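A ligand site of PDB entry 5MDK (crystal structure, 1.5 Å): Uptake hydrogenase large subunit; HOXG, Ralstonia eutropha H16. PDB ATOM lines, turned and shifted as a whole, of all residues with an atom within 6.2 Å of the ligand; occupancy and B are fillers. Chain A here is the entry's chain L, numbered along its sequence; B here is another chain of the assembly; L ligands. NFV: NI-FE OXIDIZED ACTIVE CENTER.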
ATOM      1  N   GLU A  27      27.414  23.527   4.807  1.00  0.00           N
ATOM      2  CA  GLU A  27      27.519  22.111   5.138  1.00  0.00           C
ATOM      3  C   GLU A  27      26.158  21.498   4.873  1.00  0.00           C
ATOM      4  O   GLU A  27      25.125  22.042   5.279  1.00  0.00           O
ATOM      5  CB  GLU A  27      27.932  21.904   6.599  1.00  0.00           C
ATOM      6  CG  GLU A  27      28.250  20.447   6.975  1.00  0.00           C
ATOM      7  CD  GLU A  27      27.047  19.515   6.934  1.00  0.00           C
ATOM      8  OE1 GLU A  27      25.939  19.987   7.247  1.00  0.00           O
ATOM      9  OE2 GLU A  27      27.189  18.312   6.580  1.00  0.00           O
ATOM     10  N   ILE A  74      27.130  13.867  14.075  1.00  0.00           N
ATOM     11  CA  ILE A  74      26.143  14.783  13.508  1.00  0.00           C
ATOM     12  C   ILE A  74      26.838  15.719  12.524  1.00  0.00           C
ATOM     13  O   ILE A  74      26.267  16.077  11.481  1.00  0.00           O
ATOM     14  CB  ILE A  74      25.388  15.578  14.600  1.00  0.00           C
ATOM     15  CG1 ILE A  74      24.432  14.629  15.326  1.00  0.00           C
ATOM     16  CG2 ILE A  74      24.617  16.777  14.011  1.00  0.00           C
ATOM     17  CD1 ILE A  74      23.790  15.208  16.565  1.00  0.00           C
ATOM     18  N   CYS A  75      28.069  16.143  12.857  1.00  0.00           N
ATOM     19  CA  CYS A  75      28.723  17.124  12.011  1.00  0.00           C
ATOM     20  C   CYS A  75      30.225  17.151  12.163  1.00  0.00           C
ATOM     21  O   CYS A  75      30.756  17.262  13.290  1.00  0.00           O
ATOM     22  CB  CYS A  75      28.179  18.517  12.332  1.00  0.00           C
ATOM     23  SG  CYS A  75      28.742  19.755  11.154  1.00  0.00           S
ATOM     24  N   GLY A  76      30.912  17.107  11.017  1.00  0.00           N
ATOM     25  CA  GLY A  76      32.363  17.187  10.953  1.00  0.00           C
ATOM     26  C   GLY A  76      32.932  18.588  10.786  1.00  0.00           C
ATOM     27  O   GLY A  76      34.153  18.772  10.846  1.00  0.00           O
ATOM     28  N   VAL A  77      32.045  19.575  10.602  1.00  0.00           N
ATOM     29  CA  VAL A  77      32.445  20.962  10.496  1.00  0.00           C
ATOM     30  C   VAL A  77      32.502  21.539  11.906  1.00  0.00           C
ATOM     31  O   VAL A  77      33.563  21.971  12.375  1.00  0.00           O
ATOM     32  CB  VAL A  77      31.521  21.758   9.549  1.00  0.00           C
ATOM     33  CG1 VAL A  77      31.895  23.231   9.531  1.00  0.00           C
ATOM     34  CG2 VAL A  77      31.599  21.171   8.126  1.00  0.00           C
ATOM     35  N   CYS A  78      31.400  21.487  12.644  1.00  0.00           N
ATOM     36  CA  CYS A  78      31.416  21.875  14.049  1.00  0.00           C
ATOM     37  C   CYS A  78      31.831  20.676  14.907  1.00  0.00           C
ATOM     38  O   CYS A  78      31.159  20.288  15.865  1.00  0.00           O
ATOM     39  CB  CYS A  78      30.066  22.457  14.489  1.00  0.00           C
ATOM     40  SG  CYS A  78      28.613  21.409  14.262  1.00  0.00           S
ATOM     41  N   THR A  79      32.965  20.099  14.536  1.00  0.00           N
ATOM     42  CA  THR A  79      33.390  18.809  15.082  1.00  0.00           C
ATOM     43  C   THR A  79      33.780  18.915  16.559  1.00  0.00           C
ATOM     44  O   THR A  79      34.646  19.700  16.948  1.00  0.00           O
ATOM     45  CB  THR A  79      34.528  18.177  14.258  1.00  0.00           C
ATOM     46  OG1 THR A  79      34.862  16.888  14.795  1.00  0.00           O
ATOM     47  CG2 THR A  79      35.778  19.046  14.204  1.00  0.00           C
ATOM     48  N   CYS A  81      31.620  19.771  19.062  1.00  0.00           N
ATOM     49  CA  CYS A  81      30.688  20.512  19.915  1.00  0.00           C
ATOM     50  C   CYS A  81      29.550  19.606  20.379  1.00  0.00           C
ATOM     51  O   CYS A  81      29.068  19.750  21.487  1.00  0.00           O
ATOM     52  CB  CYS A  81      30.189  21.794  19.266  1.00  0.00           C
ATOM     53  SG  CYS A  81      29.014  21.595  17.931  1.00  0.00           S
ATOM     54  N   HIS A  82      29.144  18.657  19.534  1.00  0.00           N
ATOM     55  CA  HIS A  82      28.119  17.688  19.934  1.00  0.00           C
ATOM     56  C   HIS A  82      28.639  16.690  20.963  1.00  0.00           C
ATOM     57  O   HIS A  82      27.903  16.262  21.845  1.00  0.00           O
ATOM     58  CB  HIS A  82      27.582  16.922  18.726  1.00  0.00           C
ATOM     59  CG  HIS A  82      26.726  17.752  17.823  1.00  0.00           C
ATOM     60  ND1 HIS A  82      25.467  18.158  18.179  1.00  0.00           N
ATOM     61  CD2 HIS A  82      26.963  18.287  16.600  1.00  0.00           C
ATOM     62  CE1 HIS A  82      24.940  18.888  17.210  1.00  0.00           C
ATOM     63  NE2 HIS A  82      25.830  18.986  16.241  1.00  0.00           N
ATOM     64  N   LEU A 113      37.762  25.182  18.122  1.00  0.00           N
ATOM     65  CA  LEU A 113      36.722  24.925  17.123  1.00  0.00           C
ATOM     66  C   LEU A 113      36.082  26.223  16.668  1.00  0.00           C
ATOM     67  O   LEU A 113      35.894  26.435  15.462  1.00  0.00           O
ATOM     68  CB  LEU A 113      35.639  23.998  17.667  1.00  0.00           C
ATOM     69  CG  LEU A 113      34.499  23.714  16.663  1.00  0.00           C
ATOM     70  CD1 LEU A 113      35.014  22.940  15.462  1.00  0.00           C
ATOM     71  CD2 LEU A 113      33.370  22.975  17.344  1.00  0.00           C
ATOM     72  N   ASP A 117      36.288  27.080  12.768  1.00  0.00           N
ATOM     73  CA  ASP A 117      34.996  27.092  12.081  1.00  0.00           C
ATOM     74  C   ASP A 117      34.707  28.502  11.527  1.00  0.00           C
ATOM     75  O   ASP A 117      34.368  28.648  10.362  1.00  0.00           O
ATOM     76  CB  ASP A 117      33.934  26.596  13.062  1.00  0.00           C
ATOM     77  CG  ASP A 117      32.778  25.922  12.383  1.00  0.00           C
ATOM     78  OD1 ASP A 117      32.461  26.311  11.244  1.00  0.00           O
ATOM     79  OD2 ASP A 117      32.177  25.019  13.010  1.00  0.00           O
ATOM     80  N   ALA A 528      27.811  26.679  20.639  1.00  0.00           N
ATOM     81  CA  ALA A 528      28.451  26.142  19.467  1.00  0.00           C
ATOM     82  C   ALA A 528      28.720  27.278  18.458  1.00  0.00           C
ATOM     83  O   ALA A 528      28.119  28.362  18.574  1.00  0.00           O
ATOM     84  CB  ALA A 528      27.558  25.068  18.869  1.00  0.00           C
ATOM     85  N   PRO A 529      29.602  27.044  17.477  1.00  0.00           N
ATOM     86  CA  PRO A 529      29.926  28.089  16.512  1.00  0.00           C
ATOM     87  C   PRO A 529      28.726  28.808  15.884  1.00  0.00           C
ATOM     88  O   PRO A 529      28.771  30.019  15.725  1.00  0.00           O
ATOM     89  CB  PRO A 529      30.788  27.370  15.480  1.00  0.00           C
ATOM     90  CG  PRO A 529      31.521  26.326  16.301  1.00  0.00           C
ATOM     91  CD  PRO A 529      30.498  25.875  17.320  1.00  0.00           C
ATOM     92  N   ARG A 530      27.649  28.097  15.612  1.00  0.00           N
ATOM     93  CA  ARG A 530      26.473  28.672  14.950  1.00  0.00           C
ATOM     94  C   ARG A 530      25.365  29.116  15.895  1.00  0.00           C
ATOM     95  O   ARG A 530      24.347  29.638  15.428  1.00  0.00           O
ATOM     96  CB  ARG A 530      25.937  27.674  13.932  1.00  0.00           C
ATOM     97  CG  ARG A 530      26.848  27.580  12.724  1.00  0.00           C
ATOM     98  CD  ARG A 530      26.787  26.251  12.014  1.00  0.00           C
ATOM     99  NE  ARG A 530      27.859  26.192  11.021  1.00  0.00           N
ATOM    100  CZ  ARG A 530      29.106  25.795  11.233  1.00  0.00           C
ATOM    101  NH1 ARG A 530      29.502  25.330  12.424  1.00  0.00           N
ATOM    102  NH2 ARG A 530      29.954  25.828  10.220  1.00  0.00           N
ATOM    103  N   GLY A 531      25.546  28.922  17.207  1.00  0.00           N
ATOM    104  CA  GLY A 531      24.556  29.370  18.196  1.00  0.00           C
ATOM    105  C   GLY A 531      24.315  28.418  19.355  1.00  0.00           C
ATOM    106  O   GLY A 531      25.220  27.734  19.831  1.00  0.00           O
ATOM    107  N   LEU A 533      23.277  25.288  21.283  1.00  0.00           N
ATOM    108  CA  LEU A 533      23.192  23.844  21.141  1.00  0.00           C
ATOM    109  C   LEU A 533      22.777  23.229  22.467  1.00  0.00           C
ATOM    110  O   LEU A 533      23.347  23.563  23.518  1.00  0.00           O
ATOM    111  CB  LEU A 533      24.559  23.264  20.755  1.00  0.00           C
ATOM    112  CG  LEU A 533      24.667  21.727  20.769  1.00  0.00           C
ATOM    113  CD1 LEU A 533      23.702  21.058  19.799  1.00  0.00           C
ATOM    114  CD2 LEU A 533      26.092  21.283  20.435  1.00  0.00           C
ATOM    115  N   HIS A 535      21.617  19.158  24.120  1.00  0.00           N
ATOM    116  CA  HIS A 535      21.307  17.737  24.072  1.00  0.00           C
ATOM    117  C   HIS A 535      20.588  17.405  25.370  1.00  0.00           C
ATOM    118  O   HIS A 535      21.059  17.747  26.452  1.00  0.00           O
ATOM    119  CB  HIS A 535      22.554  16.871  24.020  1.00  0.00           C
ATOM    120  CG  HIS A 535      23.299  16.924  22.720  1.00  0.00           C
ATOM    121  ND1 HIS A 535      24.184  15.936  22.362  1.00  0.00           N
ATOM    122  CD2 HIS A 535      23.316  17.833  21.722  1.00  0.00           C
ATOM    123  CE1 HIS A 535      24.723  16.236  21.196  1.00  0.00           C
ATOM    124  NE2 HIS A 535      24.212  17.385  20.793  1.00  0.00           N
ATOM    125  N   VAL A 551      19.645  22.017  17.761  1.00  0.00           N
ATOM    126  CA  VAL A 551      20.946  22.429  17.278  1.00  0.00           C
ATOM    127  C   VAL A 551      20.828  23.846  16.698  1.00  0.00           C
ATOM    128  O   VAL A 551      19.715  24.278  16.331  1.00  0.00           O
ATOM    129  CB  VAL A 551      21.435  21.339  16.292  1.00  0.00           C
ATOM    130  CG1 VAL A 551      22.827  21.570  15.762  1.00  0.00           C
ATOM    131  CG2 VAL A 551      21.346  19.967  16.944  1.00  0.00           C
ATOM    132  N   PRO A 552      21.928  24.630  16.635  1.00  0.00           N
ATOM    133  CA  PRO A 552      21.754  26.011  16.259  1.00  0.00           C
ATOM    134  C   PRO A 552      21.076  26.239  14.919  1.00  0.00           C
ATOM    135  O   PRO A 552      20.175  27.083  14.832  1.00  0.00           O
ATOM    136  CB  PRO A 552      23.176  26.565  16.262  1.00  0.00           C
ATOM    137  CG  PRO A 552      23.879  25.734  17.288  1.00  0.00           C
ATOM    138  CD  PRO A 552      23.265  24.394  17.231  1.00  0.00           C
ATOM    139  N   THR A 553      21.470  25.482  13.897  1.00  0.00           N
ATOM    140  CA  THR A 553      20.866  25.632  12.594  1.00  0.00           C
ATOM    141  C   THR A 553      19.425  25.065  12.598  1.00  0.00           C
ATOM    142  O   THR A 553      18.625  25.461  11.746  1.00  0.00           O
ATOM    143  CB  THR A 553      21.743  25.047  11.481  1.00  0.00           C
ATOM    144  OG1 THR A 553      23.026  25.691  11.526  1.00  0.00           O
ATOM    145  CG2 THR A 553      21.154  25.343  10.103  1.00  0.00           C
ATOM    146  N   THR A 554      19.068  24.214  13.555  1.00  0.00           N
ATOM    147  CA  THR A 554      17.648  23.870  13.740  1.00  0.00           C
ATOM    148  C   THR A 554      16.854  25.151  14.047  1.00  0.00           C
ATOM    149  O   THR A 554      15.802  25.395  13.434  1.00  0.00           O
ATOM    150  CB  THR A 554      17.403  22.839  14.865  1.00  0.00           C
ATOM    151  OG1 THR A 554      18.372  21.775  14.802  1.00  0.00           O
ATOM    152  CG2 THR A 554      16.007  22.239  14.752  1.00  0.00           C
ATOM    153  N   ASP A 595      26.014  30.867   8.531  1.00  0.00           N
ATOM    154  CA  ASP A 595      26.867  29.693   8.448  1.00  0.00           C
ATOM    155  C   ASP A 595      26.028  28.412   8.587  1.00  0.00           C
ATOM    156  O   ASP A 595      26.181  27.647   9.527  1.00  0.00           O
ATOM    157  CB  ASP A 595      27.951  29.859   9.531  1.00  0.00           C
ATOM    158  CG  ASP A 595      28.985  28.811   9.529  1.00  0.00           C
ATOM    159  OD1 ASP A 595      29.083  27.976   8.610  1.00  0.00           O
ATOM    160  OD2 ASP A 595      29.773  28.826  10.509  1.00  0.00           O
ATOM    161  N   PRO A 596      25.089  28.201   7.644  1.00  0.00           N
ATOM    162  CA  PRO A 596      24.188  27.073   7.785  1.00  0.00           C
ATOM    163  C   PRO A 596      24.890  25.712   7.806  1.00  0.00           C
ATOM    164  O   PRO A 596      25.739  25.442   6.947  1.00  0.00           O
ATOM    165  CB  PRO A 596      23.318  27.168   6.523  1.00  0.00           C
ATOM    166  CG  PRO A 596      23.383  28.600   6.153  1.00  0.00           C
ATOM    167  CD  PRO A 596      24.806  28.954   6.426  1.00  0.00           C
ATOM    168  N   CYS A 597      24.568  24.896   8.802  1.00  0.00           N
ATOM    169  CA  CYS A 597      25.054  23.540   8.892  1.00  0.00           C
ATOM    170  C   CYS A 597      23.838  22.634   8.847  1.00  0.00           C
ATOM    171  O   CYS A 597      23.111  22.464   9.824  1.00  0.00           O
ATOM    172  CB  CYS A 597      25.869  23.336  10.151  1.00  0.00           C
ATOM    173  SG  CYS A 597      26.691  21.734  10.087  1.00  0.00           S
ATOM    174  N   LEU A 598      23.589  22.045   7.684  1.00  0.00           N
ATOM    175  CA  LEU A 598      22.311  21.358   7.505  1.00  0.00           C
ATOM    176  C   LEU A 598      22.297  19.975   8.126  1.00  0.00           C
ATOM    177  O   LEU A 598      21.260  19.540   8.615  1.00  0.00           O
ATOM    178  CB  LEU A 598      21.894  21.360   6.027  1.00  0.00           C
ATOM    179  CG  LEU A 598      21.190  22.626   5.563  1.00  0.00           C
ATOM    180  CD1 LEU A 598      19.741  22.634   6.025  1.00  0.00           C
ATOM    181  CD2 LEU A 598      21.886  23.924   5.996  1.00  0.00           C
ATOM    182  N   ALA A 599      23.444  19.300   8.161  1.00  0.00           N
ATOM    183  CA  ALA A 599      23.567  18.028   8.870  1.00  0.00           C
ATOM    184  C   ALA A 599      23.304  18.241  10.359  1.00  0.00           C
ATOM    185  O   ALA A 599      22.589  17.470  11.005  1.00  0.00           O
ATOM    186  CB  ALA A 599      24.931  17.405   8.634  1.00  0.00           C
ATOM    187  N   CYS A 600      23.847  19.321  10.905  1.00  0.00           N
ATOM    188  CA  CYS A 600      23.525  19.733  12.268  1.00  0.00           C
ATOM    189  C   CYS A 600      22.035  19.946  12.471  1.00  0.00           C
ATOM    190  O   CYS A 600      21.449  19.498  13.455  1.00  0.00           O
ATOM    191  CB  CYS A 600      24.246  21.011  12.627  1.00  0.00           C
ATOM    192  SG  CYS A 600      25.791  20.725  13.499  1.00  0.00           S
ATOM    193  N   SER A 601      21.425  20.692  11.551  1.00  0.00           N
ATOM    194  CA  SER A 601      20.055  21.139  11.748  1.00  0.00           C
ATOM    195  C   SER A 601      19.065  19.973  11.836  1.00  0.00           C
ATOM    196  O   SER A 601      18.055  20.084  12.520  1.00  0.00           O
ATOM    197  CB  SER A 601      19.626  22.077  10.610  1.00  0.00           C
ATOM    198  OG  SER A 601      19.352  21.363   9.406  1.00  0.00           O
ATOM    199  N   CYS B  17      28.290  13.829   7.388  1.00  0.00           N
ATOM    200  CA  CYS B  17      28.563  14.884   8.332  1.00  0.00           C
ATOM    201  C   CYS B  17      29.622  15.891   7.832  1.00  0.00           C
ATOM    202  O   CYS B  17      29.847  16.924   8.495  1.00  0.00           O
ATOM    203  CB  CYS B  17      29.011  14.280   9.672  1.00  0.00           C
ATOM    204  SG  CYS B  17      30.788  13.958   9.766  1.00  0.00           S
HETATM  205 FE   NFV L   1      26.670  22.699  14.400  1.00  0.00          FE
HETATM  206 NI   NFV L   1      27.802  21.559  12.030  1.00  0.00          NI
HETATM  207  C1  NFV L   1      26.117  22.315  16.151  1.00  0.00           C
HETATM  208  O1  NFV L   1      25.820  22.114  17.216  1.00  0.00           O
HETATM  209  C2  NFV L   1      25.065  23.732  13.999  1.00  0.00           C
HETATM  210  N2  NFV L   1      24.164  24.283  13.740  1.00  0.00           N
HETATM  211  C3  NFV L   1      27.437  24.246  15.110  1.00  0.00           C
HETATM  212  N3  NFV L   1      27.951  25.231  15.511  1.00  0.00           N
HETATM  213  O4  NFV L   1      27.354  23.321  12.543  1.00  0.00           O
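The side-chain hydroxyl of Thr 554 sits close to the backbone carbonyl oxygen of Val 551, 3.2 Å away. SG of Cys 597 sits close to OE1 of Glu 27. N of Val 77 sits close to SG of Cys 75 (3.4 Å). SG of Cys 81 lies within hydrogen-bond range of O of Cys 78 (3.3 Å). A ring nitrogen (NE2) of His 535 sits at hydrogen-bond distance from a ring nitrogen (ND1) of His 82 (3.0 Å). NH2 of Arg 530 lies within salt-bridge range of OD1 of Asp 595 (2.8 Å). The side-chain hydroxyl of Thr 553 lies within hydrogen-bond range of the backbone NH of Cys 597 (3.2 Å). The guanidinium group of Arg 530 is in salt-bridge range of the side-chain carboxylate of Asp 117 (2.8 Å).
The backbone nitrogen (N) of Pro 529 sits close to a nitrogen (N3) of the ligand, 3.1 Å away. Residues that only touch the ligand: Leu 533 (3.3 Å), Val 551 (3.4 Å), Ala 528 (3.4 Å) and Pro 552 (3.4 Å). Hydrophobic or aromatic side chains that line the ligand: His 82, Ala 528, Pro 529, Leu 533, Val 551 and Pro 552. Of the 29 residues printed, 13 come within 4 Å of the ligand. Along chain A the residues within 4 Å of the ligand span positions 75 to 600.
The side-chain sulfur (SG) of Cys 597 binds a nickel atom (NI) of the ligand (2.2 Å). The side-chain hydroxyl (OG1) of Thr 553 is in hydrogen-bond range of a nitrogen (N2) of the ligand (2.9 Å). O1 of the ligand sits at hydrogen-bond distance from NE2 of His 82 (3.3 Å). A nitrogen (N2) of the ligand sits at hydrogen-bond distance from the backbone NH (N) of Thr 553. The side-chain sulfur (SG) of Cys 75 binds a nickel atom (NI) of the ligand. A nitrogen (N3) of the ligand is in hydrogen-bond range of the backbone NH (N) of Arg 530, at 2.9 Å. The guanidinium group of Arg 530 sits at hydrogen-bond distance from a nitrogen (N3) of the ligand, at 3.5 Å. The side-chain sulfur (SG) of Cys 78 binds an iron atom (FE) of the ligand, 2.3 Å away. The side-chain sulfur (SG) of Cys 81 sits at hydrogen-bond distance from an oxygen (O1) of the ligand (3.3 Å). FE of the ligand is bound by SG of Cys 600, 2.3 Å away.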
